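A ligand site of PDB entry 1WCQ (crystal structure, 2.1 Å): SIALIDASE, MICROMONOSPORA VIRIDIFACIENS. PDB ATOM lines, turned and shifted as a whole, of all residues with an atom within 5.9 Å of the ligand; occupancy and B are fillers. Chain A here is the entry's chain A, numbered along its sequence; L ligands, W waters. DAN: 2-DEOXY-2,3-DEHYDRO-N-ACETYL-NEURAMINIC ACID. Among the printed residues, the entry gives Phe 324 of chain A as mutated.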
ATOM      1  N   ARG A  22      -4.663  -3.194 -16.500  1.00  0.00           N
ATOM      2  CA  ARG A  22      -4.698  -4.555 -15.977  1.00  0.00           C
ATOM      3  C   ARG A  22      -6.074  -4.886 -15.478  1.00  0.00           C
ATOM      4  O   ARG A  22      -6.928  -4.004 -15.297  1.00  0.00           O
ATOM      5  CB  ARG A  22      -3.714  -4.756 -14.814  1.00  0.00           C
ATOM      6  CG  ARG A  22      -2.220  -4.833 -15.081  1.00  0.00           C
ATOM      7  CD  ARG A  22      -1.589  -5.497 -13.825  1.00  0.00           C
ATOM      8  NE  ARG A  22      -2.140  -6.849 -13.692  1.00  0.00           N
ATOM      9  CZ  ARG A  22      -1.980  -7.647 -12.636  1.00  0.00           C
ATOM     10  NH1 ARG A  22      -1.331  -7.220 -11.571  1.00  0.00           N
ATOM     11  NH2 ARG A  22      -2.516  -8.871 -12.619  1.00  0.00           N
ATOM     12  N   ILE A  23      -6.271  -6.185 -15.213  1.00  0.00           N
ATOM     13  CA  ILE A  23      -7.391  -6.762 -14.479  1.00  0.00           C
ATOM     14  C   ILE A  23      -8.659  -6.902 -15.305  1.00  0.00           C
ATOM     15  O   ILE A  23      -9.527  -6.058 -15.233  1.00  0.00           O
ATOM     16  CB  ILE A  23      -7.719  -6.077 -13.098  1.00  0.00           C
ATOM     17  CG1 ILE A  23      -6.434  -5.668 -12.290  1.00  0.00           C
ATOM     18  CG2 ILE A  23      -8.666  -7.067 -12.362  1.00  0.00           C
ATOM     19  CD1 ILE A  23      -5.328  -6.801 -12.042  1.00  0.00           C
ATOM     20  N   ASP A  39      -8.912  -2.079 -15.369  1.00  0.00           N
ATOM     21  CA  ASP A  39      -8.384  -0.874 -14.728  1.00  0.00           C
ATOM     22  C   ASP A  39      -7.530  -0.029 -15.691  1.00  0.00           C
ATOM     23  O   ASP A  39      -6.740  -0.591 -16.448  1.00  0.00           O
ATOM     24  CB  ASP A  39      -7.416  -1.290 -13.619  1.00  0.00           C
ATOM     25  CG  ASP A  39      -8.070  -1.806 -12.408  1.00  0.00           C
ATOM     26  OD1 ASP A  39      -9.272  -2.174 -12.398  1.00  0.00           O
ATOM     27  OD2 ASP A  39      -7.304  -1.867 -11.437  1.00  0.00           O
ATOM     28  N   ARG A  41      -4.614   2.412 -14.737  1.00  0.00           N
ATOM     29  CA  ARG A  41      -3.747   2.596 -13.559  1.00  0.00           C
ATOM     30  C   ARG A  41      -2.757   3.733 -13.796  1.00  0.00           C
ATOM     31  O   ARG A  41      -1.684   3.526 -14.379  1.00  0.00           O
ATOM     32  CB  ARG A  41      -3.001   1.292 -13.228  1.00  0.00           C
ATOM     33  CG  ARG A  41      -3.985   0.179 -12.864  1.00  0.00           C
ATOM     34  CD  ARG A  41      -3.396  -1.189 -12.697  1.00  0.00           C
ATOM     35  NE  ARG A  41      -4.327  -1.977 -11.897  1.00  0.00           N
ATOM     36  CZ  ARG A  41      -3.971  -2.936 -11.051  1.00  0.00           C
ATOM     37  NH1 ARG A  41      -2.718  -3.297 -10.952  1.00  0.00           N
ATOM     38  NH2 ARG A  41      -4.894  -3.520 -10.296  1.00  0.00           N
ATOM     39  N   ASP A  46      -1.921  -1.701  -7.984  1.00  0.00           N
ATOM     40  CA  ASP A  46      -3.207  -2.055  -7.440  1.00  0.00           C
ATOM     41  C   ASP A  46      -3.663  -0.982  -6.393  1.00  0.00           C
ATOM     42  O   ASP A  46      -2.979  -0.003  -6.173  1.00  0.00           O
ATOM     43  CB  ASP A  46      -3.116  -3.406  -6.692  1.00  0.00           C
ATOM     44  CG  ASP A  46      -2.250  -4.499  -7.412  1.00  0.00           C
ATOM     45  OD1 ASP A  46      -2.253  -4.677  -8.640  1.00  0.00           O
ATOM     46  OD2 ASP A  46      -1.564  -5.255  -6.697  1.00  0.00           O
ATOM     47  N   ALA A  47      -4.857  -1.136  -5.799  1.00  0.00           N
ATOM     48  CA  ALA A  47      -5.339  -0.230  -4.782  1.00  0.00           C
ATOM     49  C   ALA A  47      -4.243  -0.152  -3.701  1.00  0.00           C
ATOM     50  O   ALA A  47      -3.646  -1.202  -3.357  1.00  0.00           O
ATOM     51  CB  ALA A  47      -6.734  -0.721  -4.162  1.00  0.00           C
ATOM     52  N   SER A  84     -11.057  -0.161  -8.826  1.00  0.00           N
ATOM     53  CA  SER A  84     -10.097  -1.141  -9.322  1.00  0.00           C
ATOM     54  C   SER A  84     -10.623  -2.611  -9.170  1.00  0.00           C
ATOM     55  O   SER A  84     -11.415  -2.890  -8.282  1.00  0.00           O
ATOM     56  CB  SER A  84      -8.795  -0.856  -8.541  1.00  0.00           C
ATOM     57  OG  SER A  84      -7.695  -1.629  -8.974  1.00  0.00           O
ATOM     58  N   ASP A  85     -10.183  -3.541 -10.042  1.00  0.00           N
ATOM     59  CA  ASP A  85     -10.570  -4.996 -10.007  1.00  0.00           C
ATOM     60  C   ASP A  85     -12.059  -5.294 -10.331  1.00  0.00           C
ATOM     61  O   ASP A  85     -12.871  -5.617  -9.426  1.00  0.00           O
ATOM     62  CB  ASP A  85     -10.175  -5.596  -8.652  1.00  0.00           C
ATOM     63  CG  ASP A  85      -8.679  -5.862  -8.548  1.00  0.00           C
ATOM     64  OD1 ASP A  85      -7.895  -5.145  -9.219  1.00  0.00           O
ATOM     65  OD2 ASP A  85      -8.292  -6.803  -7.818  1.00  0.00           O
ATOM     66  N   VAL A 102     -13.390  -2.336  -6.264  1.00  0.00           N
ATOM     67  CA  VAL A 102     -13.073  -1.682  -5.003  1.00  0.00           C
ATOM     68  C   VAL A 102     -13.295  -0.205  -5.126  1.00  0.00           C
ATOM     69  O   VAL A 102     -13.343   0.329  -6.238  1.00  0.00           O
ATOM     70  CB  VAL A 102     -11.688  -2.036  -4.428  1.00  0.00           C
ATOM     71  CG1 VAL A 102     -11.472  -3.509  -4.520  1.00  0.00           C
ATOM     72  CG2 VAL A 102     -10.549  -1.298  -5.179  1.00  0.00           C
ATOM     73  N   PHE A 109      -5.952  -3.544  -0.062  1.00  0.00           N
ATOM     74  CA  PHE A 109      -6.456  -4.753   0.546  1.00  0.00           C
ATOM     75  C   PHE A 109      -5.671  -5.082   1.854  1.00  0.00           C
ATOM     76  O   PHE A 109      -6.270  -5.229   2.972  1.00  0.00           O
ATOM     77  CB  PHE A 109      -6.367  -5.880  -0.512  1.00  0.00           C
ATOM     78  CG  PHE A 109      -6.801  -7.219  -0.018  1.00  0.00           C
ATOM     79  CD1 PHE A 109      -8.093  -7.410   0.490  1.00  0.00           C
ATOM     80  CD2 PHE A 109      -5.935  -8.293  -0.068  1.00  0.00           C
ATOM     81  CE1 PHE A 109      -8.497  -8.636   0.943  1.00  0.00           C
ATOM     82  CE2 PHE A 109      -6.336  -9.559   0.409  1.00  0.00           C
ATOM     83  CZ  PHE A 109      -7.623  -9.718   0.912  1.00  0.00           C
ATOM     84  N   LEU A 124     -11.037  -0.313   2.685  1.00  0.00           N
ATOM     85  CA  LEU A 124     -11.171  -0.687   1.284  1.00  0.00           C
ATOM     86  C   LEU A 124     -12.651  -1.097   1.072  1.00  0.00           C
ATOM     87  O   LEU A 124     -13.144  -2.178   1.535  1.00  0.00           O
ATOM     88  CB  LEU A 124     -10.208  -1.824   0.915  1.00  0.00           C
ATOM     89  CG  LEU A 124     -10.308  -2.279  -0.559  1.00  0.00           C
ATOM     90  CD1 LEU A 124      -9.808  -1.202  -1.501  1.00  0.00           C
ATOM     91  CD2 LEU A 124      -9.496  -3.569  -0.772  1.00  0.00           C
ATOM     92  N   PHE A 157     -12.224  -7.709  -1.203  1.00  0.00           N
ATOM     93  CA  PHE A 157     -12.451  -7.274  -2.595  1.00  0.00           C
ATOM     94  C   PHE A 157     -13.098  -8.370  -3.399  1.00  0.00           C
ATOM     95  O   PHE A 157     -12.896  -9.534  -3.099  1.00  0.00           O
ATOM     96  CB  PHE A 157     -11.152  -6.802  -3.258  1.00  0.00           C
ATOM     97  CG  PHE A 157     -10.104  -7.881  -3.458  1.00  0.00           C
ATOM     98  CD1 PHE A 157      -9.725  -8.260  -4.758  1.00  0.00           C
ATOM     99  CD2 PHE A 157      -9.455  -8.448  -2.358  1.00  0.00           C
ATOM    100  CE1 PHE A 157      -8.718  -9.227  -4.978  1.00  0.00           C
ATOM    101  CE2 PHE A 157      -8.424  -9.416  -2.558  1.00  0.00           C
ATOM    102  CZ  PHE A 157      -8.058  -9.802  -3.897  1.00  0.00           C
ATOM    103  N   PHE A 188      -6.897 -15.026   5.105  1.00  0.00           N
ATOM    104  CA  PHE A 188      -7.614 -14.619   3.876  1.00  0.00           C
ATOM    105  C   PHE A 188      -8.638 -15.730   3.670  1.00  0.00           C
ATOM    106  O   PHE A 188      -8.247 -16.919   3.641  1.00  0.00           O
ATOM    107  CB  PHE A 188      -6.677 -14.608   2.644  1.00  0.00           C
ATOM    108  CG  PHE A 188      -5.650 -13.470   2.621  1.00  0.00           C
ATOM    109  CD1 PHE A 188      -5.378 -12.695   3.768  1.00  0.00           C
ATOM    110  CD2 PHE A 188      -4.922 -13.204   1.443  1.00  0.00           C
ATOM    111  CE1 PHE A 188      -4.427 -11.682   3.717  1.00  0.00           C
ATOM    112  CE2 PHE A 188      -3.949 -12.201   1.410  1.00  0.00           C
ATOM    113  CZ  PHE A 188      -3.709 -11.436   2.541  1.00  0.00           C
ATOM    114  N   ASP A 213      -7.857 -16.569  -1.642  1.00  0.00           N
ATOM    115  CA  ASP A 213      -7.557 -15.372  -2.343  1.00  0.00           C
ATOM    116  C   ASP A 213      -8.624 -15.297  -3.421  1.00  0.00           C
ATOM    117  O   ASP A 213      -9.598 -15.989  -3.324  1.00  0.00           O
ATOM    118  CB  ASP A 213      -6.156 -15.450  -2.924  1.00  0.00           C
ATOM    119  CG  ASP A 213      -5.501 -14.051  -3.043  1.00  0.00           C
ATOM    120  OD1 ASP A 213      -6.076 -13.201  -3.759  1.00  0.00           O
ATOM    121  OD2 ASP A 213      -4.461 -13.814  -2.369  1.00  0.00           O
ATOM    122  N   GLU A 214      -8.479 -14.427  -4.410  1.00  0.00           N
ATOM    123  CA  GLU A 214      -9.423 -14.383  -5.545  1.00  0.00           C
ATOM    124  C   GLU A 214      -9.971 -15.735  -5.934  1.00  0.00           C
ATOM    125  O   GLU A 214      -9.204 -16.603  -6.342  1.00  0.00           O
ATOM    126  CB  GLU A 214      -8.694 -13.833  -6.780  1.00  0.00           C
ATOM    127  CG  GLU A 214      -8.234 -12.313  -6.628  1.00  0.00           C
ATOM    128  CD  GLU A 214      -7.173 -11.903  -7.681  1.00  0.00           C
ATOM    129  OE1 GLU A 214      -6.323 -12.750  -8.043  1.00  0.00           O
ATOM    130  OE2 GLU A 214      -7.211 -10.743  -8.159  1.00  0.00           O
ATOM    131  N   ARG A 230      -7.512 -19.136  -6.065  1.00  0.00           N
ATOM    132  CA  ARG A 230      -6.091 -18.834  -5.980  1.00  0.00           C
ATOM    133  C   ARG A 230      -5.664 -19.154  -4.552  1.00  0.00           C
ATOM    134  O   ARG A 230      -6.381 -18.861  -3.596  1.00  0.00           O
ATOM    135  CB  ARG A 230      -5.923 -17.300  -6.293  1.00  0.00           C
ATOM    136  CG  ARG A 230      -4.554 -16.599  -5.941  1.00  0.00           C
ATOM    137  CD  ARG A 230      -4.561 -15.140  -6.369  1.00  0.00           C
ATOM    138  NE  ARG A 230      -3.359 -14.418  -5.893  1.00  0.00           N
ATOM    139  CZ  ARG A 230      -2.891 -13.296  -6.437  1.00  0.00           C
ATOM    140  NH1 ARG A 230      -3.527 -12.741  -7.475  1.00  0.00           N
ATOM    141  NH2 ARG A 230      -1.814 -12.729  -5.926  1.00  0.00           N
ATOM    142  N   SER A 232      -3.270 -18.054  -1.712  1.00  0.00           N
ATOM    143  CA  SER A 232      -2.348 -17.030  -1.183  1.00  0.00           C
ATOM    144  C   SER A 232      -1.264 -17.664  -0.317  1.00  0.00           C
ATOM    145  O   SER A 232      -0.246 -17.024  -0.069  1.00  0.00           O
ATOM    146  CB  SER A 232      -3.118 -15.959  -0.425  1.00  0.00           C
ATOM    147  OG  SER A 232      -3.860 -16.479   0.723  1.00  0.00           O
ATOM    148  N   THR A 263      -0.138 -18.785  -8.162  1.00  0.00           N
ATOM    149  CA  THR A 263      -0.777 -17.739  -7.312  1.00  0.00           C
ATOM    150  C   THR A 263      -1.140 -16.555  -8.189  1.00  0.00           C
ATOM    151  O   THR A 263      -0.456 -15.486  -8.193  1.00  0.00           O
ATOM    152  CB  THR A 263       0.115 -17.294  -6.133  1.00  0.00           C
ATOM    153  OG1 THR A 263       0.795 -18.431  -5.600  1.00  0.00           O
ATOM    154  CG2 THR A 263      -0.718 -16.620  -5.045  1.00  0.00           C
ATOM    155  N   ASN A 264      -2.249 -16.744  -8.902  1.00  0.00           N
ATOM    156  CA  ASN A 264      -2.678 -15.886  -9.992  1.00  0.00           C
ATOM    157  C   ASN A 264      -4.211 -16.073 -10.090  1.00  0.00           C
ATOM    158  O   ASN A 264      -4.721 -17.121  -9.690  1.00  0.00           O
ATOM    159  CB  ASN A 264      -1.971 -16.384 -11.282  1.00  0.00           C
ATOM    160  CG  ASN A 264      -2.185 -15.454 -12.484  1.00  0.00           C
ATOM    161  OD1 ASN A 264      -2.458 -14.247 -12.354  1.00  0.00           O
ATOM    162  ND2 ASN A 264      -2.011 -16.017 -13.664  1.00  0.00           N
ATOM    163  N   ARG A 296       3.792 -16.775 -14.330  1.00  0.00           N
ATOM    164  CA  ARG A 296       2.545 -16.405 -14.985  1.00  0.00           C
ATOM    165  C   ARG A 296       2.779 -16.462 -16.498  1.00  0.00           C
ATOM    166  O   ARG A 296       3.069 -15.461 -17.180  1.00  0.00           O
ATOM    167  CB  ARG A 296       2.039 -15.032 -14.493  1.00  0.00           C
ATOM    168  CG  ARG A 296       1.508 -15.033 -13.066  1.00  0.00           C
ATOM    169  CD  ARG A 296       1.292 -13.568 -12.529  1.00  0.00           C
ATOM    170  NE  ARG A 296       0.781 -13.574 -11.165  1.00  0.00           N
ATOM    171  CZ  ARG A 296       0.081 -12.611 -10.597  1.00  0.00           C
ATOM    172  NH1 ARG A 296      -0.197 -11.482 -11.253  1.00  0.00           N
ATOM    173  NH2 ARG A 296      -0.362 -12.788  -9.353  1.00  0.00           N
ATOM    174  N   PHE A 324      -3.721 -12.607 -15.496  1.00  0.00           N
ATOM    175  CA  PHE A 324      -5.170 -12.799 -15.290  1.00  0.00           C
ATOM    176  C   PHE A 324      -5.881 -13.114 -16.641  1.00  0.00           C
ATOM    177  O   PHE A 324      -5.518 -12.591 -17.700  1.00  0.00           O
ATOM    178  CB  PHE A 324      -5.777 -11.519 -14.671  1.00  0.00           C
ATOM    179  CG  PHE A 324      -5.476 -11.296 -13.176  1.00  0.00           C
ATOM    180  CD1 PHE A 324      -4.321 -11.779 -12.572  1.00  0.00           C
ATOM    181  CD2 PHE A 324      -6.349 -10.511 -12.421  1.00  0.00           C
ATOM    182  CE1 PHE A 324      -4.066 -11.550 -11.206  1.00  0.00           C
ATOM    183  CE2 PHE A 324      -6.139 -10.275 -11.079  1.00  0.00           C
ATOM    184  CZ  PHE A 324      -4.993 -10.787 -10.447  1.00  0.00           C
ATOM    185  N   GLU A 340      -4.301 -11.007 -19.695  1.00  0.00           N
ATOM    186  CA  GLU A 340      -3.160 -10.091 -19.599  1.00  0.00           C
ATOM    187  C   GLU A 340      -1.874 -10.701 -20.209  1.00  0.00           C
ATOM    188  O   GLU A 340      -1.220 -11.530 -19.582  1.00  0.00           O
ATOM    189  CB  GLU A 340      -2.894  -9.711 -18.139  1.00  0.00           C
ATOM    190  CG  GLU A 340      -4.100  -9.053 -17.430  1.00  0.00           C
ATOM    191  CD  GLU A 340      -3.770  -8.817 -16.000  1.00  0.00           C
ATOM    192  OE1 GLU A 340      -3.322  -9.762 -15.298  1.00  0.00           O
ATOM    193  OE2 GLU A 340      -3.932  -7.660 -15.575  1.00  0.00           O
HETATM  194  C1  DAN L   1      -2.075  -9.755  -8.736  1.00  0.00           C
HETATM  195  C2  DAN L   1      -3.236  -8.914  -8.097  1.00  0.00           C
HETATM  196  C3  DAN L   1      -3.950  -7.976  -8.826  1.00  0.00           C
HETATM  197  C4  DAN L   1      -5.119  -7.272  -8.119  1.00  0.00           C
HETATM  198  C5  DAN L   1      -4.973  -7.199  -6.653  1.00  0.00           C
HETATM  199  C6  DAN L   1      -4.772  -8.606  -6.149  1.00  0.00           C
HETATM  200  C7  DAN L   1      -4.514  -8.666  -4.645  1.00  0.00           C
HETATM  201  C8  DAN L   1      -4.058 -10.022  -4.248  1.00  0.00           C
HETATM  202  C9  DAN L   1      -4.029 -10.120  -2.732  1.00  0.00           C
HETATM  203  C10 DAN L   1      -6.270  -5.622  -5.214  1.00  0.00           C
HETATM  204  C11 DAN L   1      -7.640  -5.454  -4.531  1.00  0.00           C
HETATM  205  N5  DAN L   1      -6.261  -6.730  -6.140  1.00  0.00           N
HETATM  206  O1A DAN L   1      -1.771  -9.566  -9.950  1.00  0.00           O
HETATM  207  O1B DAN L   1      -1.500 -10.577  -8.003  1.00  0.00           O
HETATM  208  O4  DAN L   1      -5.532  -6.018  -8.702  1.00  0.00           O
HETATM  209  O6  DAN L   1      -3.595  -9.165  -6.779  1.00  0.00           O
HETATM  210  O7  DAN L   1      -3.511  -7.738  -4.139  1.00  0.00           O
HETATM  211  O8  DAN L   1      -4.921 -11.019  -4.803  1.00  0.00           O
HETATM  212  O9  DAN L   1      -3.591 -11.447  -2.555  1.00  0.00           O
HETATM  213  O10 DAN L   1      -5.241  -5.834  -4.289  1.00  0.00           O
HETATM  214  O   HOH W   1      -4.383  -3.748  -2.546  1.00  0.00           O
HETATM  215  O   HOH W   2      -1.011  -7.992  -5.146  1.00  0.00           O
HETATM  216  O   HOH W   3      -1.256 -11.202  -0.786  1.00  0.00           O
HETATM  217  O   HOH W   4      -6.364  -3.210  -7.011  1.00  0.00           O
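The side-chain carboxylate (OD2) of Asp 213 is in hydrogen-bond range of an oxygen (O9) of the ligand, at 2.5 Å.
An oxygen (O4) of the ligand lies within hydrogen-bond range of the side-chain carboxylate of Asp 85.
The guanidinium group (NH1) of Arg 296 lies within salt-bridge range of an oxygen (O1A) of the ligand.
NH2 of Arg 22 lies within salt-bridge range of O1A of the ligand, 2.9 Å away.
The guanidinium group of Arg 230 is in salt-bridge range of an oxygen (O1B) of the ligand, 3.0 Å away.
The guanidinium group (NH2) of Arg 41 lies within hydrogen-bond range of an oxygen (O4) of the ligand (3.0 Å).
OD1 of Asp 213 lies within salt-bridge range of NE of Arg 230, at 3.7 Å.
The side-chain carboxylate (OD1) of Asp 85 is in salt-bridge range of the guanidinium group (NH2) of Arg 41 (3.6 Å).
N of Asp 85 lies within hydrogen-bond range of OD1 of Asp 39.
The backbone carbonyl oxygen of Thr 263 is in hydrogen-bond range of the guanidinium group of Arg 296, 2.9 Å away.
The backbone carbonyl oxygen of Arg 22 is in hydrogen-bond range of the backbone NH of Asp 39.
The guanidinium group (NE) of Arg 22 lies within salt-bridge range of the side-chain carboxylate (OE2) of Glu 340, at 2.7 Å.
The backbone carbonyl oxygen (O) of Phe 324 lies within hydrogen-bond range of the backbone NH (N) of Glu 340 (2.8 Å).
The backbone NH (N) of Ile 23 lies within hydrogen-bond range of the side-chain carboxylate (OE2) of Glu 340, 2.8 Å away.
Residues that only touch the ligand: Ile 23 (3.4 Å), Asp 46 (3.5 Å), Phe 109 (3.8 Å), Phe 157 (3.5 Å), Glu 214 (3.8 Å) and Phe 324 (3.3 Å).
12 residues have an atom within 4 Å of the ligand: Arg 22, Ile 23, Arg 41, Asp 46, Asp 85, Phe 109, Phe 157, Asp 213, Glu 214, Arg 230, Arg 296 and Phe 324.
Water W2 bridges O7 of the ligand (2.7 Å) and OD2 of Asp 46 (3.2 Å).
Water W1 lies within hydrogen-bond range of O of Ala 47 (2.8 Å), O10 of the ligand (2.9 Å) and N of Phe 109 (2.9 Å).
Water W4 lies within hydrogen-bond range of N of Ala 47, OG of Ser 84, OD1 of Asp 85 and O4 of the ligand.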
